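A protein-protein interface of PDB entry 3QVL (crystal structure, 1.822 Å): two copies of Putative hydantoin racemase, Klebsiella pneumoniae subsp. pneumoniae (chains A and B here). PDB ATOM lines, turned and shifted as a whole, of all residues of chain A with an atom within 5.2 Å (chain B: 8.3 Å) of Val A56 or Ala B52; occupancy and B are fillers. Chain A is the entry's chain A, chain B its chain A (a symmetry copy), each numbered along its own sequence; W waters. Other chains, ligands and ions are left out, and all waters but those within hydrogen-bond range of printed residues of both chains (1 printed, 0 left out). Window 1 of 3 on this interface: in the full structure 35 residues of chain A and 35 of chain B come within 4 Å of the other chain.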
ATOM      1  N   ALA A  52      -8.419  29.106   5.527  1.00  0.00           N
ATOM      2  CA  ALA A  52      -7.422  28.573   6.455  1.00  0.00           C
ATOM      3  C   ALA A  52      -6.070  28.378   5.772  1.00  0.00           C
ATOM      4  O   ALA A  52      -5.024  28.660   6.360  1.00  0.00           O
ATOM      5  CB  ALA A  52      -7.907  27.268   7.071  1.00  0.00           C
ATOM      6  N   ILE A  53      -6.104  27.899   4.529  1.00  0.00           N
ATOM      7  CA  ILE A  53      -4.898  27.741   3.716  1.00  0.00           C
ATOM      8  C   ILE A  53      -4.305  29.108   3.374  1.00  0.00           C
ATOM      9  O   ILE A  53      -3.098  29.324   3.523  1.00  0.00           O
ATOM     10  CB  ILE A  53      -5.184  26.930   2.426  1.00  0.00           C
ATOM     11  CG1 ILE A  53      -5.532  25.480   2.779  1.00  0.00           C
ATOM     12  CG2 ILE A  53      -3.987  26.973   1.474  1.00  0.00           C
ATOM     13  CD1 ILE A  53      -6.091  24.678   1.626  1.00  0.00           C
ATOM     14  N   ALA A  54      -5.167  30.026   2.937  1.00  0.00           N
ATOM     15  CA  ALA A  54      -4.759  31.380   2.563  1.00  0.00           C
ATOM     16  C   ALA A  54      -4.109  32.139   3.719  1.00  0.00           C
ATOM     17  O   ALA A  54      -3.161  32.897   3.507  1.00  0.00           O
ATOM     18  CB  ALA A  54      -5.944  32.157   2.019  1.00  0.00           C
ATOM     19  N   ALA A  55      -4.620  31.923   4.932  1.00  0.00           N
ATOM     20  CA  ALA A  55      -4.098  32.573   6.137  1.00  0.00           C
ATOM     21  C   ALA A  55      -2.608  32.298   6.361  1.00  0.00           C
ATOM     22  O   ALA A  55      -1.850  33.209   6.698  1.00  0.00           O
ATOM     23  CB  ALA A  55      -4.911  32.163   7.359  1.00  0.00           C
ATOM     24  N   VAL A  56      -2.199  31.045   6.167  1.00  0.00           N
ATOM     25  CA  VAL A  56      -0.793  30.650   6.310  1.00  0.00           C
ATOM     26  C   VAL A  56       0.060  31.226   5.174  1.00  0.00           C
ATOM     27  O   VAL A  56       1.202  31.639   5.395  1.00  0.00           O
ATOM     28  CB  VAL A  56      -0.640  29.109   6.433  1.00  0.00           C
ATOM     29  CG1 VAL A  56       0.814  28.671   6.265  1.00  0.00           C
ATOM     30  CG2 VAL A  56      -1.171  28.641   7.780  1.00  0.00           C
ATOM     31  N   GLY A  57      -0.509  31.267   3.970  1.00  0.00           N
ATOM     32  CA  GLY A  57       0.140  31.899   2.822  1.00  0.00           C
ATOM     33  C   GLY A  57       0.390  33.380   3.039  1.00  0.00           C
ATOM     34  O   GLY A  57       1.433  33.905   2.640  1.00  0.00           O
ATOM     35  N   VAL A  58      -0.572  34.051   3.673  1.00  0.00           N
ATOM     36  CA  VAL A  58      -0.421  35.451   4.075  1.00  0.00           C
ATOM     37  C   VAL A  58       0.769  35.607   5.026  1.00  0.00           C
ATOM     38  O   VAL A  58       1.611  36.485   4.829  1.00  0.00           O
ATOM     39  CB  VAL A  58      -1.720  36.006   4.731  1.00  0.00           C
ATOM     40  CG1 VAL A  58      -1.462  37.336   5.434  1.00  0.00           C
ATOM     41  CG2 VAL A  58      -2.818  36.166   3.691  1.00  0.00           C
ATOM     42  N   LEU A  59       0.838  34.735   6.032  1.00  0.00           N
ATOM     43  CA  LEU A  59       1.904  34.770   7.038  1.00  0.00           C
ATOM     44  C   LEU A  59       3.296  34.577   6.439  1.00  0.00           C
ATOM     45  O   LEU A  59       4.259  35.205   6.883  1.00  0.00           O
ATOM     46  CB  LEU A  59       1.650  33.735   8.140  1.00  0.00           C
ATOM     47  CG  LEU A  59       0.457  33.973   9.073  1.00  0.00           C
ATOM     48  CD1 LEU A  59       0.271  32.790  10.009  1.00  0.00           C
ATOM     49  CD2 LEU A  59       0.616  35.267   9.867  1.00  0.00           C
ATOM     50  N   GLU A  60       3.388  33.705   5.435  1.00  0.00           N
ATOM     51  CA  GLU A  60       4.633  33.487   4.700  1.00  0.00           C
ATOM     52  C   GLU A  60       5.106  34.778   4.031  1.00  0.00           C
ATOM     53  O   GLU A  60       6.299  35.092   4.048  1.00  0.00           O
ATOM     54  CB  GLU A  60       4.458  32.377   3.660  1.00  0.00           C
ATOM     55  N   ALA A  85      -3.459  37.287  12.982  1.00  0.00           N
ATOM     56  CA  ALA A  85      -2.211  36.524  12.946  1.00  0.00           C
ATOM     57  C   ALA A  85      -1.099  37.348  12.300  1.00  0.00           C
ATOM     58  O   ALA A  85       0.032  37.372  12.792  1.00  0.00           O
ATOM     59  CB  ALA A  85      -2.410  35.215  12.196  1.00  0.00           C
ATOM     60  N   PHE A 239       6.057  24.766   8.710  1.00  0.00           N
ATOM     61  CA  PHE A 239       5.847  26.050   9.382  1.00  0.00           C
ATOM     62  C   PHE A 239       7.123  26.680   9.949  1.00  0.00           C
ATOM     63  O   PHE A 239       7.092  27.817  10.424  1.00  0.00           O
ATOM     64  CB  PHE A 239       4.809  25.902  10.502  1.00  0.00           C
ATOM     65  CG  PHE A 239       3.514  25.280  10.060  1.00  0.00           C
ATOM     66  CD1 PHE A 239       2.598  26.004   9.300  1.00  0.00           C
ATOM     67  CD2 PHE A 239       3.200  23.974  10.419  1.00  0.00           C
ATOM     68  CE1 PHE A 239       1.395  25.430   8.895  1.00  0.00           C
ATOM     69  CE2 PHE A 239       1.998  23.391  10.022  1.00  0.00           C
ATOM     70  CZ  PHE A 239       1.094  24.121   9.258  1.00  0.00           C
ATOM     71  N   LEU A 242       8.242  30.422   9.193  1.00  0.00           N
ATOM     72  CA  LEU A 242       7.272  31.505   9.398  1.00  0.00           C
ATOM     73  C   LEU A 242       7.715  32.594  10.376  1.00  0.00           C
ATOM     74  O   LEU A 242       7.336  33.757  10.218  1.00  0.00           O
ATOM     75  CB  LEU A 242       5.910  30.943   9.826  1.00  0.00           C
ATOM     76  CG  LEU A 242       5.066  30.203   8.783  1.00  0.00           C
ATOM     77  CD1 LEU A 242       3.844  29.578   9.436  1.00  0.00           C
ATOM     78  CD2 LEU A 242       4.649  31.119   7.637  1.00  0.00           C
ATOM     79  N   VAL B  42       2.774  23.869  16.005  1.00  0.00           N
ATOM     80  CA  VAL B  42       3.184  24.643  17.168  1.00  0.00           C
ATOM     81  C   VAL B  42       2.933  23.837  18.456  1.00  0.00           C
ATOM     82  O   VAL B  42       1.889  23.200  18.583  1.00  0.00           O
ATOM     83  CB  VAL B  42       2.457  26.029  17.169  1.00  0.00           C
ATOM     84  CG1 VAL B  42       0.950  25.890  17.426  1.00  0.00           C
ATOM     85  CG2 VAL B  42       3.095  26.987  18.142  1.00  0.00           C
ATOM     86  N   ILE B  45      -0.754  26.757  21.669  1.00  0.00           N
ATOM     87  CA  ILE B  45      -1.450  27.830  20.970  1.00  0.00           C
ATOM     88  C   ILE B  45      -1.706  29.002  21.917  1.00  0.00           C
ATOM     89  O   ILE B  45      -2.513  28.903  22.845  1.00  0.00           O
ATOM     90  CB  ILE B  45      -2.758  27.328  20.320  1.00  0.00           C
ATOM     91  CG1 ILE B  45      -2.463  26.142  19.395  1.00  0.00           C
ATOM     92  CG2 ILE B  45      -3.431  28.448  19.538  1.00  0.00           C
ATOM     93  CD1 ILE B  45      -3.602  25.155  19.270  1.00  0.00           C
ATOM     94  N   GLY B  47      -2.109  32.617  20.898  1.00  0.00           N
ATOM     95  CA  GLY B  47      -2.347  33.806  20.089  1.00  0.00           C
ATOM     96  C   GLY B  47      -2.868  33.486  18.703  1.00  0.00           C
ATOM     97  O   GLY B  47      -3.088  32.321  18.364  1.00  0.00           O
ATOM     98  N   HIS B  48      -3.050  34.532  17.901  1.00  0.00           N
ATOM     99  CA  HIS B  48      -3.674  34.421  16.583  1.00  0.00           C
ATOM    100  C   HIS B  48      -2.761  33.758  15.551  1.00  0.00           C
ATOM    101  O   HIS B  48      -3.229  32.999  14.698  1.00  0.00           O
ATOM    102  CB  HIS B  48      -4.136  35.799  16.099  1.00  0.00           C
ATOM    103  CG  HIS B  48      -4.909  36.569  17.126  1.00  0.00           C
ATOM    104  ND1 HIS B  48      -6.279  36.483  17.248  1.00  0.00           N
ATOM    105  CD2 HIS B  48      -4.501  37.437  18.082  1.00  0.00           C
ATOM    106  CE1 HIS B  48      -6.681  37.263  18.236  1.00  0.00           C
ATOM    107  NE2 HIS B  48      -5.622  37.853  18.759  1.00  0.00           N
ATOM    108  N   PHE B  49      -1.464  34.057  15.636  1.00  0.00           N
ATOM    109  CA  PHE B  49      -0.442  33.439  14.787  1.00  0.00           C
ATOM    110  C   PHE B  49      -0.402  31.926  15.002  1.00  0.00           C
ATOM    111  O   PHE B  49      -0.421  31.155  14.038  1.00  0.00           O
ATOM    112  CB  PHE B  49       0.925  34.080  15.068  1.00  0.00           C
ATOM    113  CG  PHE B  49       2.081  33.426  14.358  1.00  0.00           C
ATOM    114  CD1 PHE B  49       2.405  33.776  13.052  1.00  0.00           C
ATOM    115  CD2 PHE B  49       2.870  32.483  15.013  1.00  0.00           C
ATOM    116  CE1 PHE B  49       3.485  33.181  12.399  1.00  0.00           C
ATOM    117  CE2 PHE B  49       3.952  31.885  14.371  1.00  0.00           C
ATOM    118  CZ  PHE B  49       4.258  32.235  13.063  1.00  0.00           C
ATOM    119  N   ASP B  50      -0.365  31.516  16.270  1.00  0.00           N
ATOM    120  CA  ASP B  50      -0.390  30.103  16.642  1.00  0.00           C
ATOM    121  C   ASP B  50      -1.662  29.410  16.149  1.00  0.00           C
ATOM    122  O   ASP B  50      -1.609  28.275  15.673  1.00  0.00           O
ATOM    123  CB  ASP B  50      -0.266  29.939  18.160  1.00  0.00           C
ATOM    124  CG  ASP B  50       1.082  30.392  18.701  1.00  0.00           C
ATOM    125  OD1 ASP B  50       2.041  30.545  17.913  1.00  0.00           O
ATOM    126  OD2 ASP B  50       1.179  30.591  19.931  1.00  0.00           O
ATOM    127  N   GLU B  51      -2.796  30.104  16.261  1.00  0.00           N
ATOM    128  CA  GLU B  51      -4.092  29.577  15.822  1.00  0.00           C
ATOM    129  C   GLU B  51      -4.148  29.287  14.325  1.00  0.00           C
ATOM    130  O   GLU B  51      -4.703  28.267  13.910  1.00  0.00           O
ATOM    131  CB  GLU B  51      -5.229  30.531  16.196  1.00  0.00           C
ATOM    132  CG  GLU B  51      -5.668  30.438  17.643  1.00  0.00           C
ATOM    133  CD  GLU B  51      -7.170  30.543  17.804  1.00  0.00           C
ATOM    134  OE1 GLU B  51      -7.779  31.478  17.240  1.00  0.00           O
ATOM    135  OE2 GLU B  51      -7.742  29.682  18.497  1.00  0.00           O
ATOM    136  N   ALA B  52      -3.580  30.189  13.525  1.00  0.00           N
ATOM    137  CA  ALA B  52      -3.554  30.040  12.071  1.00  0.00           C
ATOM    138  C   ALA B  52      -2.759  28.806  11.649  1.00  0.00           C
ATOM    139  O   ALA B  52      -3.155  28.093  10.726  1.00  0.00           O
ATOM    140  CB  ALA B  52      -2.991  31.294  11.415  1.00  0.00           C
ATOM    141  N   ILE B  53      -1.642  28.566  12.334  1.00  0.00           N
ATOM    142  CA  ILE B  53      -0.823  27.376  12.104  1.00  0.00           C
ATOM    143  C   ILE B  53      -1.580  26.119  12.531  1.00  0.00           C
ATOM    144  O   ILE B  53      -1.632  25.133  11.787  1.00  0.00           O
ATOM    145  CB  ILE B  53       0.538  27.472  12.841  1.00  0.00           C
ATOM    146  CG1 ILE B  53       1.396  28.582  12.226  1.00  0.00           C
ATOM    147  CG2 ILE B  53       1.284  26.136  12.793  1.00  0.00           C
ATOM    148  CD1 ILE B  53       2.621  28.942  13.036  1.00  0.00           C
ATOM    149  N   ALA B  54      -2.180  26.172  13.720  1.00  0.00           N
ATOM    150  CA  ALA B  54      -2.939  25.052  14.275  1.00  0.00           C
ATOM    151  C   ALA B  54      -4.116  24.645  13.391  1.00  0.00           C
ATOM    152  O   ALA B  54      -4.417  23.456  13.269  1.00  0.00           O
ATOM    153  CB  ALA B  54      -3.420  25.384  15.677  1.00  0.00           C
ATOM    154  N   ALA B  55      -4.767  25.633  12.776  1.00  0.00           N
ATOM    155  CA  ALA B  55      -5.911  25.396  11.891  1.00  0.00           C
ATOM    156  C   ALA B  55      -5.576  24.458  10.728  1.00  0.00           C
ATOM    157  O   ALA B  55      -6.360  23.564  10.404  1.00  0.00           O
ATOM    158  CB  ALA B  55      -6.467  26.718  11.373  1.00  0.00           C
ATOM    159  N   VAL B  56      -4.413  24.665  10.112  1.00  0.00           N
ATOM    160  CA  VAL B  56      -3.951  23.818   9.007  1.00  0.00           C
ATOM    161  C   VAL B  56      -3.569  22.419   9.508  1.00  0.00           C
ATOM    162  O   VAL B  56      -3.828  21.419   8.832  1.00  0.00           O
ATOM    163  CB  VAL B  56      -2.798  24.490   8.212  1.00  0.00           C
ATOM    164  CG1 VAL B  56      -2.106  23.500   7.275  1.00  0.00           C
ATOM    165  CG2 VAL B  56      -3.337  25.669   7.416  1.00  0.00           C
ATOM    166  N   GLY B  57      -2.972  22.361  10.697  1.00  0.00           N
ATOM    167  CA  GLY B  57      -2.661  21.089  11.352  1.00  0.00           C
ATOM    168  C   GLY B  57      -3.904  20.269  11.645  1.00  0.00           C
ATOM    169  O   GLY B  57      -3.894  19.042  11.502  1.00  0.00           O
ATOM    170  N   VAL B  58      -4.973  20.949  12.057  1.00  0.00           N
ATOM    171  CA  VAL B  58      -6.281  20.319  12.250  1.00  0.00           C
ATOM    172  C   VAL B  58      -6.772  19.697  10.940  1.00  0.00           C
ATOM    173  O   VAL B  58      -7.194  18.539  10.920  1.00  0.00           O
ATOM    174  CB  VAL B  58      -7.331  21.326  12.804  1.00  0.00           C
ATOM    175  CG1 VAL B  58      -8.747  20.768  12.697  1.00  0.00           C
ATOM    176  CG2 VAL B  58      -7.017  21.688  14.247  1.00  0.00           C
ATOM    177  N   LEU B  59      -6.687  20.468   9.855  1.00  0.00           N
ATOM    178  CA  LEU B  59      -7.138  20.024   8.532  1.00  0.00           C
ATOM    179  C   LEU B  59      -6.389  18.792   8.029  1.00  0.00           C
ATOM    180  O   LEU B  59      -6.981  17.916   7.393  1.00  0.00           O
ATOM    181  CB  LEU B  59      -7.040  21.162   7.510  1.00  0.00           C
ATOM    182  CG  LEU B  59      -7.992  22.351   7.682  1.00  0.00           C
ATOM    183  CD1 LEU B  59      -7.667  23.442   6.673  1.00  0.00           C
ATOM    184  CD2 LEU B  59      -9.452  21.923   7.557  1.00  0.00           C
ATOM    185  N   PRO B  81      -9.622  26.257  16.646  1.00  0.00           N
ATOM    186  CA  PRO B  81      -9.019  26.698  15.388  1.00  0.00           C
ATOM    187  C   PRO B  81      -9.428  25.836  14.197  1.00  0.00           C
ATOM    188  O   PRO B  81      -9.418  24.603  14.281  1.00  0.00           O
ATOM    189  CB  PRO B  81      -7.513  26.570  15.653  1.00  0.00           C
ATOM    190  CG  PRO B  81      -7.400  25.542  16.704  1.00  0.00           C
ATOM    191  CD  PRO B  81      -8.608  25.724  17.573  1.00  0.00           C
ATOM    192  N   GLY B  82      -9.801  26.502  13.108  1.00  0.00           N
ATOM    193  CA  GLY B  82     -10.187  25.837  11.867  1.00  0.00           C
ATOM    194  C   GLY B  82     -11.482  25.049  11.933  1.00  0.00           C
ATOM    195  O   GLY B  82     -11.667  24.107  11.163  1.00  0.00           O
ATOM    196  N   ILE B 124      -9.355  35.914  22.228  1.00  0.00           N
ATOM    197  CA  ILE B 124      -9.786  34.805  21.374  1.00  0.00           C
ATOM    198  C   ILE B 124     -11.066  34.173  21.929  1.00  0.00           C
ATOM    199  O   ILE B 124     -11.993  33.868  21.174  1.00  0.00           O
ATOM    200  CB  ILE B 124      -8.662  33.742  21.206  1.00  0.00           C
ATOM    201  CG1 ILE B 124      -7.436  34.366  20.522  1.00  0.00           C
ATOM    202  CG2 ILE B 124      -9.161  32.529  20.414  1.00  0.00           C
ATOM    203  CD1 ILE B 124      -6.171  33.520  20.587  1.00  0.00           C
ATOM    204  N   GLN B 238       2.983  22.744   0.153  1.00  0.00           N
ATOM    205  CA  GLN B 238       2.725  22.068   1.428  1.00  0.00           C
ATOM    206  C   GLN B 238       1.257  21.674   1.642  1.00  0.00           C
ATOM    207  O   GLN B 238       0.952  20.838   2.495  1.00  0.00           O
ATOM    208  CB  GLN B 238       3.215  22.944   2.590  1.00  0.00           C
ATOM    209  CG  GLN B 238       2.417  24.232   2.788  1.00  0.00           C
ATOM    210  CD  GLN B 238       3.141  25.268   3.626  1.00  0.00           C
ATOM    211  OE1 GLN B 238       2.795  25.495   4.785  1.00  0.00           O
ATOM    212  NE2 GLN B 238       4.150  25.905   3.041  1.00  0.00           N
ATOM    213  N   PHE B 239       0.359  22.276   0.862  1.00  0.00           N
ATOM    214  CA  PHE B 239      -1.082  22.090   1.040  1.00  0.00           C
ATOM    215  C   PHE B 239      -1.697  21.020   0.132  1.00  0.00           C
ATOM    216  O   PHE B 239      -2.874  20.687   0.280  1.00  0.00           O
ATOM    217  CB  PHE B 239      -1.819  23.420   0.834  1.00  0.00           C
ATOM    218  CG  PHE B 239      -1.290  24.552   1.670  1.00  0.00           C
ATOM    219  CD1 PHE B 239      -1.553  24.611   3.037  1.00  0.00           C
ATOM    220  CD2 PHE B 239      -0.543  25.569   1.088  1.00  0.00           C
ATOM    221  CE1 PHE B 239      -1.067  25.663   3.812  1.00  0.00           C
ATOM    222  CE2 PHE B 239      -0.055  26.627   1.853  1.00  0.00           C
ATOM    223  CZ  PHE B 239      -0.318  26.673   3.218  1.00  0.00           C
HETATM  224  O   HOH W   1      -5.053  29.020   9.039  1.00  0.00           O
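Among the printed residues, merely in contact across the chains: Ala A52 with Val B56, Ala A52 with Leu B59, Ile A53 with Phe B239, Val A56 with Ala B52, Val A56 with Val B56, Val A56 with Phe B239, Leu A59 with Phe B49, Leu A59 with Ala B52, Ala A85 with His B48, Ala A85 with Phe B49, Phe A239 with Ile B53, Phe A239 with Val B56, Leu A242 with Phe B49 and Leu A242 with Ile B53.
Of the printed residues of chain B, Ala A52 touches Val B56 and Leu B59.
Printed residues of chain B within 4 Å of Ile A53: Phe B239 (3.6 Å).
Val A56 touches three residues of chain B.
Of the printed residues of chain B, Leu A242 touches Phe B49 and Ile B53.
Of the printed residues of chain A, Phe B49 touches Leu A59, Ala A85 and Leu A242.
Of chain A, only Val A56 and Leu A59 come within 4 Å of Ala B52.
Printed residues of chain A within 4 Å of Val B56: Ala A52, Val A56 and Phe A239.
Ile B124 touches none of the printed residues of chain A.
The nearest printed residue of chain A that does not touch His B48 is Leu A59 (5.9 Å).
Of the 20 printed residues of chain B, 7 touch a printed residue of chain A.
Printed residues of chain B that touch a printed residue of chain A: His B48, Phe B49, Ala B52, Ile B53, Val B56, Leu B59 and Phe B239.
Of the 12 printed residues of chain A, 7 touch a printed residue of chain B.
Printed residues of chain A that touch a printed residue of chain B: Ala A52, Ile A53, Val A56, Leu A59, Ala A85, Phe A239 and Leu A242.
Hydrophobic or aromatic side chains of chain A that line the printed part of chain B: Ala A52, Ile A53, Val A56, Leu A59, Ala A85, Phe A239 and Leu A242.
Among the printed residues, no Asp or Glu carboxylate lies within 4 Å of a Lys or Arg side-chain nitrogen of the other chain.
Ala A52 touches Val B56, and with the chains exchanged Val A56 touches Ala B52.
Ala A52 touches Leu B59, and with the chains exchanged Leu A59 touches Ala B52.
Val B56 touches its own counterpart, Val A56.
Val A56 touches Phe B239, and with the chains exchanged Phe A239 touches Val B56.
Water W1 lies within hydrogen-bond range of O of Ala A52 (2.7 Å) and O of Ala B52 (2.7 Å).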
